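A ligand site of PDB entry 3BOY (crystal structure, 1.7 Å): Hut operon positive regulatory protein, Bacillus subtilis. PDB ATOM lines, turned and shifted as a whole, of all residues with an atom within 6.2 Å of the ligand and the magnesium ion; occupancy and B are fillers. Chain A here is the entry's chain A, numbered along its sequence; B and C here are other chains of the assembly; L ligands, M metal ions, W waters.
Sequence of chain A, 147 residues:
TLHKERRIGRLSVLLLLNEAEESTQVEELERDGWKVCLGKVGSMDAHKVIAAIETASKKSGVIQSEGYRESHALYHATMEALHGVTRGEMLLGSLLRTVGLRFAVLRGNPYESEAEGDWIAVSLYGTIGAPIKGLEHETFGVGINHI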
ATOM      1  N   VAL A  85      15.927  30.885  -4.079  1.00  0.00           N
ATOM      2  CA  VAL A  85      14.986  29.857  -4.471  1.00  0.00           C
ATOM      3  C   VAL A  85      14.234  30.237  -5.757  1.00  0.00           C
ATOM      4  O   VAL A  85      14.074  29.376  -6.619  1.00  0.00           O
ATOM      5  CB  VAL A  85      13.983  29.546  -3.316  1.00  0.00           C
ATOM      6  CG1 VAL A  85      12.840  28.683  -3.805  1.00  0.00           C
ATOM      7  CG2 VAL A  85      14.763  28.913  -2.140  1.00  0.00           C
ATOM      8  N   THR A  86      13.811  31.504  -5.876  1.00  0.00           N
ATOM      9  CA  THR A  86      12.958  31.937  -7.005  1.00  0.00           C
ATOM     10  C   THR A  86      13.690  32.588  -8.182  1.00  0.00           C
ATOM     11  O   THR A  86      13.173  32.643  -9.311  1.00  0.00           O
ATOM     12  CB  THR A  86      11.838  32.866  -6.533  1.00  0.00           C
ATOM     13  OG1 THR A  86      12.360  34.000  -5.841  1.00  0.00           O
ATOM     14  CG2 THR A  86      10.863  32.109  -5.568  1.00  0.00           C
ATOM     15  N   ARG A  87      14.860  33.144  -7.892  1.00  0.00           N
ATOM     16  CA  ARG A  87      15.774  33.547  -8.985  1.00  0.00           C
ATOM     17  C   ARG A  87      15.123  34.540  -9.985  1.00  0.00           C
ATOM     18  O   ARG A  87      15.288  34.444 -11.202  1.00  0.00           O
ATOM     19  CB  ARG A  87      16.417  32.325  -9.651  1.00  0.00           C
ATOM     20  CG  ARG A  87      17.454  31.643  -8.792  1.00  0.00           C
ATOM     21  CD  ARG A  87      17.536  30.172  -9.074  1.00  0.00           C
ATOM     22  NE  ARG A  87      16.202  29.562  -8.812  1.00  0.00           N
ATOM     23  CZ  ARG A  87      15.434  28.959  -9.702  1.00  0.00           C
ATOM     24  NH1 ARG A  87      15.799  28.824 -10.986  1.00  0.00           N
ATOM     25  NH2 ARG A  87      14.249  28.514  -9.292  1.00  0.00           N
ATOM     26  N   LEU A  95       3.342  31.380 -11.562  1.00  0.00           N
ATOM     27  CA  LEU A  95       4.210  31.062 -12.680  1.00  0.00           C
ATOM     28  C   LEU A  95       4.254  29.564 -12.940  1.00  0.00           C
ATOM     29  O   LEU A  95       5.225  29.023 -13.466  1.00  0.00           O
ATOM     30  CB  LEU A  95       5.645  31.613 -12.459  1.00  0.00           C
ATOM     31  CG  LEU A  95       5.742  33.129 -12.293  1.00  0.00           C
ATOM     32  CD1 LEU A  95       7.242  33.400 -12.079  1.00  0.00           C
ATOM     33  CD2 LEU A  95       5.192  33.868 -13.501  1.00  0.00           C
ATOM     34  N   LEU A  96       3.161  28.881 -12.571  1.00  0.00           N
ATOM     35  CA  LEU A  96       3.062  27.421 -12.828  1.00  0.00           C
ATOM     36  C   LEU A  96       4.269  26.633 -12.280  1.00  0.00           C
ATOM     37  O   LEU A  96       4.797  25.705 -12.909  1.00  0.00           O
ATOM     38  CB  LEU A  96       2.799  27.162 -14.322  1.00  0.00           C
ATOM     39  CG  LEU A  96       2.035  25.885 -14.672  1.00  0.00           C
ATOM     40  CD1 LEU A  96       0.656  25.867 -13.950  1.00  0.00           C
ATOM     41  CD2 LEU A  96       1.832  25.808 -16.172  1.00  0.00           C
ATOM     42  N   ARG A  97       4.710  26.988 -11.083  1.00  0.00           N
ATOM     43  CA  ARG A  97       5.703  26.172 -10.407  1.00  0.00           C
ATOM     44  C   ARG A  97       5.419  25.943  -8.926  1.00  0.00           C
ATOM     45  O   ARG A  97       4.685  26.706  -8.258  1.00  0.00           O
ATOM     46  CB  ARG A  97       7.112  26.719 -10.647  1.00  0.00           C
ATOM     47  CG  ARG A  97       7.340  28.105 -10.142  1.00  0.00           C
ATOM     48  CD  ARG A  97       8.856  28.530 -10.365  1.00  0.00           C
ATOM     49  NE  ARG A  97       9.017  29.896  -9.864  1.00  0.00           N
ATOM     50  CZ  ARG A  97      10.123  30.621  -9.979  1.00  0.00           C
ATOM     51  NH1 ARG A  97      11.224  30.110 -10.583  1.00  0.00           N
ATOM     52  NH2 ARG A  97      10.109  31.863  -9.527  1.00  0.00           N
ATOM     53  N   THR A  98       6.014  24.880  -8.414  1.00  0.00           N
ATOM     54  CA  THR A  98       5.773  24.498  -7.019  1.00  0.00           C
ATOM     55  C   THR A  98       7.110  24.242  -6.375  1.00  0.00           C
ATOM     56  O   THR A  98       8.048  23.813  -7.080  1.00  0.00           O
ATOM     57  CB  THR A  98       4.888  23.164  -6.987  1.00  0.00           C
ATOM     58  OG1 THR A  98       4.789  22.655  -5.647  1.00  0.00           O
ATOM     59  CG2 THR A  98       5.499  22.059  -7.877  1.00  0.00           C
ATOM     60  N   ILE A 128      12.196  22.657  -6.970  1.00  0.00           N
ATOM     61  CA  ILE A 128      11.214  23.552  -7.592  1.00  0.00           C
ATOM     62  C   ILE A 128      10.930  22.974  -8.976  1.00  0.00           C
ATOM     63  O   ILE A 128      11.831  22.424  -9.624  1.00  0.00           O
ATOM     64  CB  ILE A 128      11.820  24.994  -7.649  1.00  0.00           C
ATOM     65  CG1 ILE A 128      10.765  26.040  -8.061  1.00  0.00           C
ATOM     66  CG2 ILE A 128      13.095  25.004  -8.531  1.00  0.00           C
ATOM     67  CD1 ILE A 128      11.204  27.530  -7.810  1.00  0.00           C
ATOM     68  N   GLY A 129       9.688  23.052  -9.421  1.00  0.00           N
ATOM     69  CA  GLY A 129       9.373  22.456 -10.713  1.00  0.00           C
ATOM     70  C   GLY A 129       7.985  22.717 -11.176  1.00  0.00           C
ATOM     71  O   GLY A 129       7.239  23.417 -10.512  1.00  0.00           O
ATOM     72  N   ALA A 130       7.649  22.161 -12.328  1.00  0.00           N
ATOM     73  CA  ALA A 130       6.267  22.084 -12.793  1.00  0.00           C
ATOM     74  C   ALA A 130       5.492  21.257 -11.749  1.00  0.00           C
ATOM     75  O   ALA A 130       6.105  20.490 -11.015  1.00  0.00           O
ATOM     76  CB  ALA A 130       6.209  21.428 -14.129  1.00  0.00           C
ATOM     77  N   PRO A 131       4.183  21.483 -11.639  1.00  0.00           N
ATOM     78  CA  PRO A 131       3.377  20.666 -10.726  1.00  0.00           C
ATOM     79  C   PRO A 131       3.116  19.232 -11.208  1.00  0.00           C
ATOM     80  O   PRO A 131       1.986  18.765 -11.169  1.00  0.00           O
ATOM     81  CB  PRO A 131       2.057  21.428 -10.621  1.00  0.00           C
ATOM     82  CG  PRO A 131       1.964  22.224 -11.856  1.00  0.00           C
ATOM     83  CD  PRO A 131       3.369  22.523 -12.308  1.00  0.00           C
ATOM     84  N   LEU A 135       9.290  16.501 -12.614  1.00  0.00           N
ATOM     85  CA  LEU A 135       9.573  17.606 -13.538  1.00  0.00           C
ATOM     86  C   LEU A 135      10.070  18.760 -12.676  1.00  0.00           C
ATOM     87  O   LEU A 135       9.391  19.767 -12.512  1.00  0.00           O
ATOM     88  CB  LEU A 135       8.338  18.027 -14.316  1.00  0.00           C
ATOM     89  CG  LEU A 135       7.749  17.101 -15.398  1.00  0.00           C
ATOM     90  CD1 LEU A 135       6.795  17.856 -16.271  1.00  0.00           C
ATOM     91  CD2 LEU A 135       8.825  16.493 -16.213  1.00  0.00           C
ATOM     92  N   GLU A 136      11.255  18.569 -12.119  1.00  0.00           N
ATOM     93  CA  GLU A 136      11.799  19.462 -11.085  1.00  0.00           C
ATOM     94  C   GLU A 136      13.294  19.363 -11.006  1.00  0.00           C
ATOM     95  O   GLU A 136      13.881  18.362 -11.445  1.00  0.00           O
ATOM     96  CB  GLU A 136      11.212  19.058  -9.719  1.00  0.00           C
ATOM     97  CG  GLU A 136      11.586  17.603  -9.302  1.00  0.00           C
ATOM     98  CD  GLU A 136      10.591  16.992  -8.308  1.00  0.00           C
ATOM     99  OE1 GLU A 136       9.380  17.136  -8.527  1.00  0.00           O
ATOM    100  OE2 GLU A 136      11.039  16.402  -7.298  1.00  0.00           O
ATOM    101  N   HIS A 137      13.932  20.417 -10.479  1.00  0.00           N
ATOM    102  CA  HIS A 137      15.336  20.382 -10.098  1.00  0.00           C
ATOM    103  C   HIS A 137      15.515  20.994  -8.726  1.00  0.00           C
ATOM    104  O   HIS A 137      14.549  21.529  -8.146  1.00  0.00           O
ATOM    105  CB  HIS A 137      16.278  21.019 -11.180  1.00  0.00           C
ATOM    106  CG  HIS A 137      16.000  22.475 -11.490  1.00  0.00           C
ATOM    107  ND1 HIS A 137      16.225  23.482 -10.573  1.00  0.00           N
ATOM    108  CD2 HIS A 137      15.594  23.078 -12.636  1.00  0.00           C
ATOM    109  CE1 HIS A 137      15.919  24.651 -11.124  1.00  0.00           C
ATOM    110  NE2 HIS A 137      15.545  24.438 -12.374  1.00  0.00           N
ATOM    111  N   GLU B  54       2.947  25.487 -23.242  1.00  0.00           N
ATOM    112  CA  GLU B  54       3.493  24.171 -22.999  1.00  0.00           C
ATOM    113  C   GLU B  54       2.603  23.105 -23.657  1.00  0.00           C
ATOM    114  O   GLU B  54       3.106  22.197 -24.330  1.00  0.00           O
ATOM    115  CB  GLU B  54       3.546  23.870 -21.518  1.00  0.00           C
ATOM    116  CG  GLU B  54       4.324  22.577 -21.209  1.00  0.00           C
ATOM    117  CD  GLU B  54       4.075  22.087 -19.802  1.00  0.00           C
ATOM    118  OE1 GLU B  54       3.926  22.935 -18.885  1.00  0.00           O
ATOM    119  OE2 GLU B  54       4.017  20.838 -19.610  1.00  0.00           O
ATOM    120  N   TYR B  68      11.983  15.718 -18.403  1.00  0.00           N
ATOM    121  CA  TYR B  68      12.036  17.104 -17.913  1.00  0.00           C
ATOM    122  C   TYR B  68      12.862  18.010 -18.841  1.00  0.00           C
ATOM    123  O   TYR B  68      12.449  19.145 -19.097  1.00  0.00           O
ATOM    124  CB  TYR B  68      12.596  17.143 -16.519  1.00  0.00           C
ATOM    125  CG  TYR B  68      12.528  18.488 -15.828  1.00  0.00           C
ATOM    126  CD1 TYR B  68      11.383  19.313 -15.949  1.00  0.00           C
ATOM    127  CD2 TYR B  68      13.578  18.926 -15.036  1.00  0.00           C
ATOM    128  CE1 TYR B  68      11.311  20.577 -15.289  1.00  0.00           C
ATOM    129  CE2 TYR B  68      13.530  20.184 -14.373  1.00  0.00           C
ATOM    130  CZ  TYR B  68      12.379  20.974 -14.482  1.00  0.00           C
ATOM    131  OH  TYR B  68      12.304  22.218 -13.809  1.00  0.00           O
ATOM    132  N   SER B  71      10.966  20.254 -21.391  1.00  0.00           N
ATOM    133  CA  SER B  71      10.036  21.057 -20.615  1.00  0.00           C
ATOM    134  C   SER B  71      10.807  22.186 -19.884  1.00  0.00           C
ATOM    135  O   SER B  71      10.341  23.337 -19.878  1.00  0.00           O
ATOM    136  CB  SER B  71       9.297  20.167 -19.628  1.00  0.00           C
ATOM    137  OG  SER B  71       8.351  19.368 -20.354  1.00  0.00           O
ATOM    138  N   HIS B  72      11.965  21.834 -19.337  1.00  0.00           N
ATOM    139  CA  HIS B  72      12.793  22.845 -18.640  1.00  0.00           C
ATOM    140  C   HIS B  72      13.229  23.923 -19.619  1.00  0.00           C
ATOM    141  O   HIS B  72      13.138  25.141 -19.347  1.00  0.00           O
ATOM    142  CB  HIS B  72      14.030  22.197 -18.028  1.00  0.00           C
ATOM    143  CG  HIS B  72      14.786  23.125 -17.117  1.00  0.00           C
ATOM    144  ND1 HIS B  72      15.985  23.693 -17.482  1.00  0.00           N
ATOM    145  CD2 HIS B  72      14.534  23.544 -15.858  1.00  0.00           C
ATOM    146  CE1 HIS B  72      16.430  24.455 -16.507  1.00  0.00           C
ATOM    147  NE2 HIS B  72      15.562  24.381 -15.505  1.00  0.00           N
ATOM    148  N   TYR B  75      10.243  26.093 -20.535  1.00  0.00           N
ATOM    149  CA  TYR B  75       9.738  26.923 -19.422  1.00  0.00           C
ATOM    150  C   TYR B  75      10.581  28.227 -19.369  1.00  0.00           C
ATOM    151  O   TYR B  75      10.068  29.327 -19.306  1.00  0.00           O
ATOM    152  CB  TYR B  75       9.866  26.187 -18.089  1.00  0.00           C
ATOM    153  CG  TYR B  75       9.330  26.984 -16.919  1.00  0.00           C
ATOM    154  CD1 TYR B  75       7.946  27.102 -16.676  1.00  0.00           C
ATOM    155  CD2 TYR B  75      10.201  27.711 -16.096  1.00  0.00           C
ATOM    156  CE1 TYR B  75       7.461  27.846 -15.591  1.00  0.00           C
ATOM    157  CE2 TYR B  75       9.725  28.474 -15.017  1.00  0.00           C
ATOM    158  CZ  TYR B  75       8.344  28.555 -14.772  1.00  0.00           C
ATOM    159  OH  TYR B  75       7.815  29.266 -13.677  1.00  0.00           O
ATOM    160  N   HIS B  76      11.880  28.050 -19.424  1.00  0.00           N
ATOM    161  CA  HIS B  76      12.772  29.213 -19.294  1.00  0.00           C
ATOM    162  C   HIS B  76      12.715  30.088 -20.519  1.00  0.00           C
ATOM    163  O   HIS B  76      12.746  31.305 -20.398  1.00  0.00           O
ATOM    164  CB  HIS B  76      14.156  28.743 -18.969  1.00  0.00           C
ATOM    165  CG  HIS B  76      14.328  28.402 -17.540  1.00  0.00           C
ATOM    166  ND1 HIS B  76      14.497  29.359 -16.573  1.00  0.00           N
ATOM    167  CD2 HIS B  76      14.356  27.205 -16.914  1.00  0.00           C
ATOM    168  CE1 HIS B  76      14.659  28.777 -15.391  1.00  0.00           C
ATOM    169  NE2 HIS B  76      14.556  27.467 -15.577  1.00  0.00           N
ATOM    170  N   GLU C  80      21.704  32.540 -12.473  1.00  0.00           N
ATOM    171  CA  GLU C  80      20.828  32.010 -11.409  1.00  0.00           C
ATOM    172  C   GLU C  80      21.551  31.925 -10.046  1.00  0.00           C
ATOM    173  O   GLU C  80      21.019  32.350  -9.021  1.00  0.00           O
ATOM    174  CB  GLU C  80      20.164  30.695 -11.864  1.00  0.00           C
ATOM    175  CG  GLU C  80      19.190  30.901 -13.083  1.00  0.00           C
ATOM    176  CD  GLU C  80      18.144  29.783 -13.288  1.00  0.00           C
ATOM    177  OE1 GLU C  80      18.196  28.833 -12.535  1.00  0.00           O
ATOM    178  N   TRP C 119      23.337  17.904 -16.897  1.00  0.00           N
ATOM    179  CA  TRP C 119      22.926  19.187 -16.309  1.00  0.00           C
ATOM    180  C   TRP C 119      24.129  19.793 -15.647  1.00  0.00           C
ATOM    181  O   TRP C 119      25.132  19.120 -15.373  1.00  0.00           O
ATOM    182  CB  TRP C 119      21.817  18.943 -15.277  1.00  0.00           C
ATOM    183  CG  TRP C 119      20.535  18.505 -15.914  1.00  0.00           C
ATOM    184  CD1 TRP C 119      20.301  17.341 -16.602  1.00  0.00           C
ATOM    185  CD2 TRP C 119      19.298  19.205 -15.903  1.00  0.00           C
ATOM    186  NE1 TRP C 119      19.017  17.305 -17.044  1.00  0.00           N
ATOM    187  CE2 TRP C 119      18.367  18.432 -16.623  1.00  0.00           C
ATOM    188  CE3 TRP C 119      18.872  20.447 -15.354  1.00  0.00           C
ATOM    189  CZ2 TRP C 119      17.035  18.842 -16.823  1.00  0.00           C
ATOM    190  CZ3 TRP C 119      17.587  20.845 -15.549  1.00  0.00           C
ATOM    191  CH2 TRP C 119      16.655  20.050 -16.274  1.00  0.00           C
ATOM    192  N   ILE C 144      21.073  26.046 -11.469  1.00  0.00           N
ATOM    193  CA  ILE C 144      21.077  24.712 -12.131  1.00  0.00           C
ATOM    194  C   ILE C 144      20.467  24.818 -13.509  1.00  0.00           C
ATOM    195  O   ILE C 144      19.470  25.500 -13.696  1.00  0.00           O
ATOM    196  CB  ILE C 144      20.306  23.725 -11.239  1.00  0.00           C
ATOM    197  CG1 ILE C 144      21.206  23.384 -10.019  1.00  0.00           C
ATOM    198  CG2 ILE C 144      20.001  22.415 -12.006  1.00  0.00           C
ATOM    199  CD1 ILE C 144      20.553  22.759  -8.802  1.00  0.00           C
ATOM    200  N   ASN C 145      21.088  24.203 -14.515  1.00  0.00           N
ATOM    201  CA  ASN C 145      20.584  24.268 -15.869  1.00  0.00           C
ATOM    202  C   ASN C 145      20.831  22.961 -16.645  1.00  0.00           C
ATOM    203  O   ASN C 145      21.699  22.188 -16.261  1.00  0.00           O
ATOM    204  CB  ASN C 145      21.242  25.459 -16.598  1.00  0.00           C
ATOM    205  CG  ASN C 145      20.424  26.007 -17.736  1.00  0.00           C
ATOM    206  OD1 ASN C 145      19.253  25.622 -17.967  1.00  0.00           O
ATOM    207  ND2 ASN C 145      21.009  26.955 -18.444  1.00  0.00           N
HETATM  208  C1  LIG L   1      12.092  26.090 -13.155  1.00  0.00           C
HETATM  209  C2  LIG L   1      12.902  26.988 -12.267  1.00  0.00           C
HETATM  210  O1  LIG L   1      14.107  27.062 -12.520  1.00  0.00           O
HETATM  211  C3  LIG L   1      10.940  25.399 -12.431  1.00  0.00           C
HETATM  212  C4  LIG L   1       9.924  24.851 -13.382  1.00  0.00           C
HETATM  213  N1  LIG L   1      10.190  23.779 -14.211  1.00  0.00           N
HETATM  214  C5  LIG L   1       8.672  25.273 -13.697  1.00  0.00           C
HETATM  215  C6  LIG L   1       9.138  23.554 -14.992  1.00  0.00           C
HETATM  216  N2  LIG L   1       8.209  24.449 -14.698  1.00  0.00           N
HETATM  217  O2  LIG L   1      12.403  27.606 -11.321  1.00  0.00           O
HETATM  218 MG    MG M   1      15.059  25.923 -13.924  1.00  0.00          MG
HETATM  219  O   HOH W   1       5.414  24.506 -15.279  1.00  0.00           O
HETATM  220  O   HOH W   2      16.939  26.794 -13.788  1.00  0.00           O
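An oxygen (O2) of the ligand lies within salt-bridge range of the guanidinium group of Arg 97 (2.9 Å).
The side-chain hydroxyl (OH) of Tyr 68 of chain B lies within hydrogen-bond range of a nitrogen (N1) of the ligand (2.7 Å).
The backbone NH (N) of Ala 130 sits close to a nitrogen (N2) of the ligand (3.3 Å).
The guanidinium group (NH2) of Arg 87 is in salt-bridge range of an oxygen (O2) of the ligand (2.9 Å).
The backbone NH of Thr 98 is in hydrogen-bond range of the backbone carbonyl oxygen of Gly 129, at 2.8 Å.
NH1 of Arg 87 is in salt-bridge range of OE1 of Glu 80 of chain C (2.9 Å).
O of Leu 95 lies within hydrogen-bond range of OH of Tyr 75 of chain B, 2.6 Å away.
The guanidinium group (NH2) of Arg 87 sits at hydrogen-bond distance from the backbone carbonyl oxygen (O) of Val 85.
The backbone carbonyl oxygen (O) of His 137 lies within hydrogen-bond range of the backbone NH (N) of Ile 128.
N of Ala 130 lies within hydrogen-bond range of O of Leu 135, at 3.0 Å.
The backbone carbonyl oxygen (O) of Thr 86 lies within hydrogen-bond range of the guanidinium group (NH2) of Arg 97 (3.2 Å).
Merely in contact with the ligand: Tyr 75 of chain B (3.3 Å), Gly 129 (3.6 Å), Ile 128 (3.7 Å) and Leu 96 (3.98 Å).
Hydrophobic or aromatic side chains within 4 Å of the ligand: Ile 128, Ala 130, His 137, Tyr 68 of chain B, Tyr 75 of chain B and His 76 of chain B.
Along chain A the residues within 4 Å of the ligand span positions 87 to 137.
The nearest printed residue that does not touch the ligand is His 72 of chain B (4.3 Å).
The nearest printed residue that does not touch the magnesium ion is Arg 87 (4.2 Å).
An oxygen (O1) of the ligand binds the magnesium ion (2.0 Å).
The magnesium ion is bound by water W2 (2.1 Å).
A ring nitrogen (NE2) of His 137 is bound to the magnesium ion, 2.2 Å away.
The magnesium ion is bound by NE2 of His 72 of chain B, 2.3 Å away.
The magnesium ion is bound by a ring nitrogen (NE2) of His 76 of chain B.
Water W2 bridges OE1 of Glu 80 of chain C (2.7 Å) and O of Ile 144 of chain C (2.8 Å).
Water W1 lies within hydrogen-bond range of the backbone carbonyl oxygen of Leu 96 (2.7 Å) and a nitrogen (N2) of the ligand (2.9 Å).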
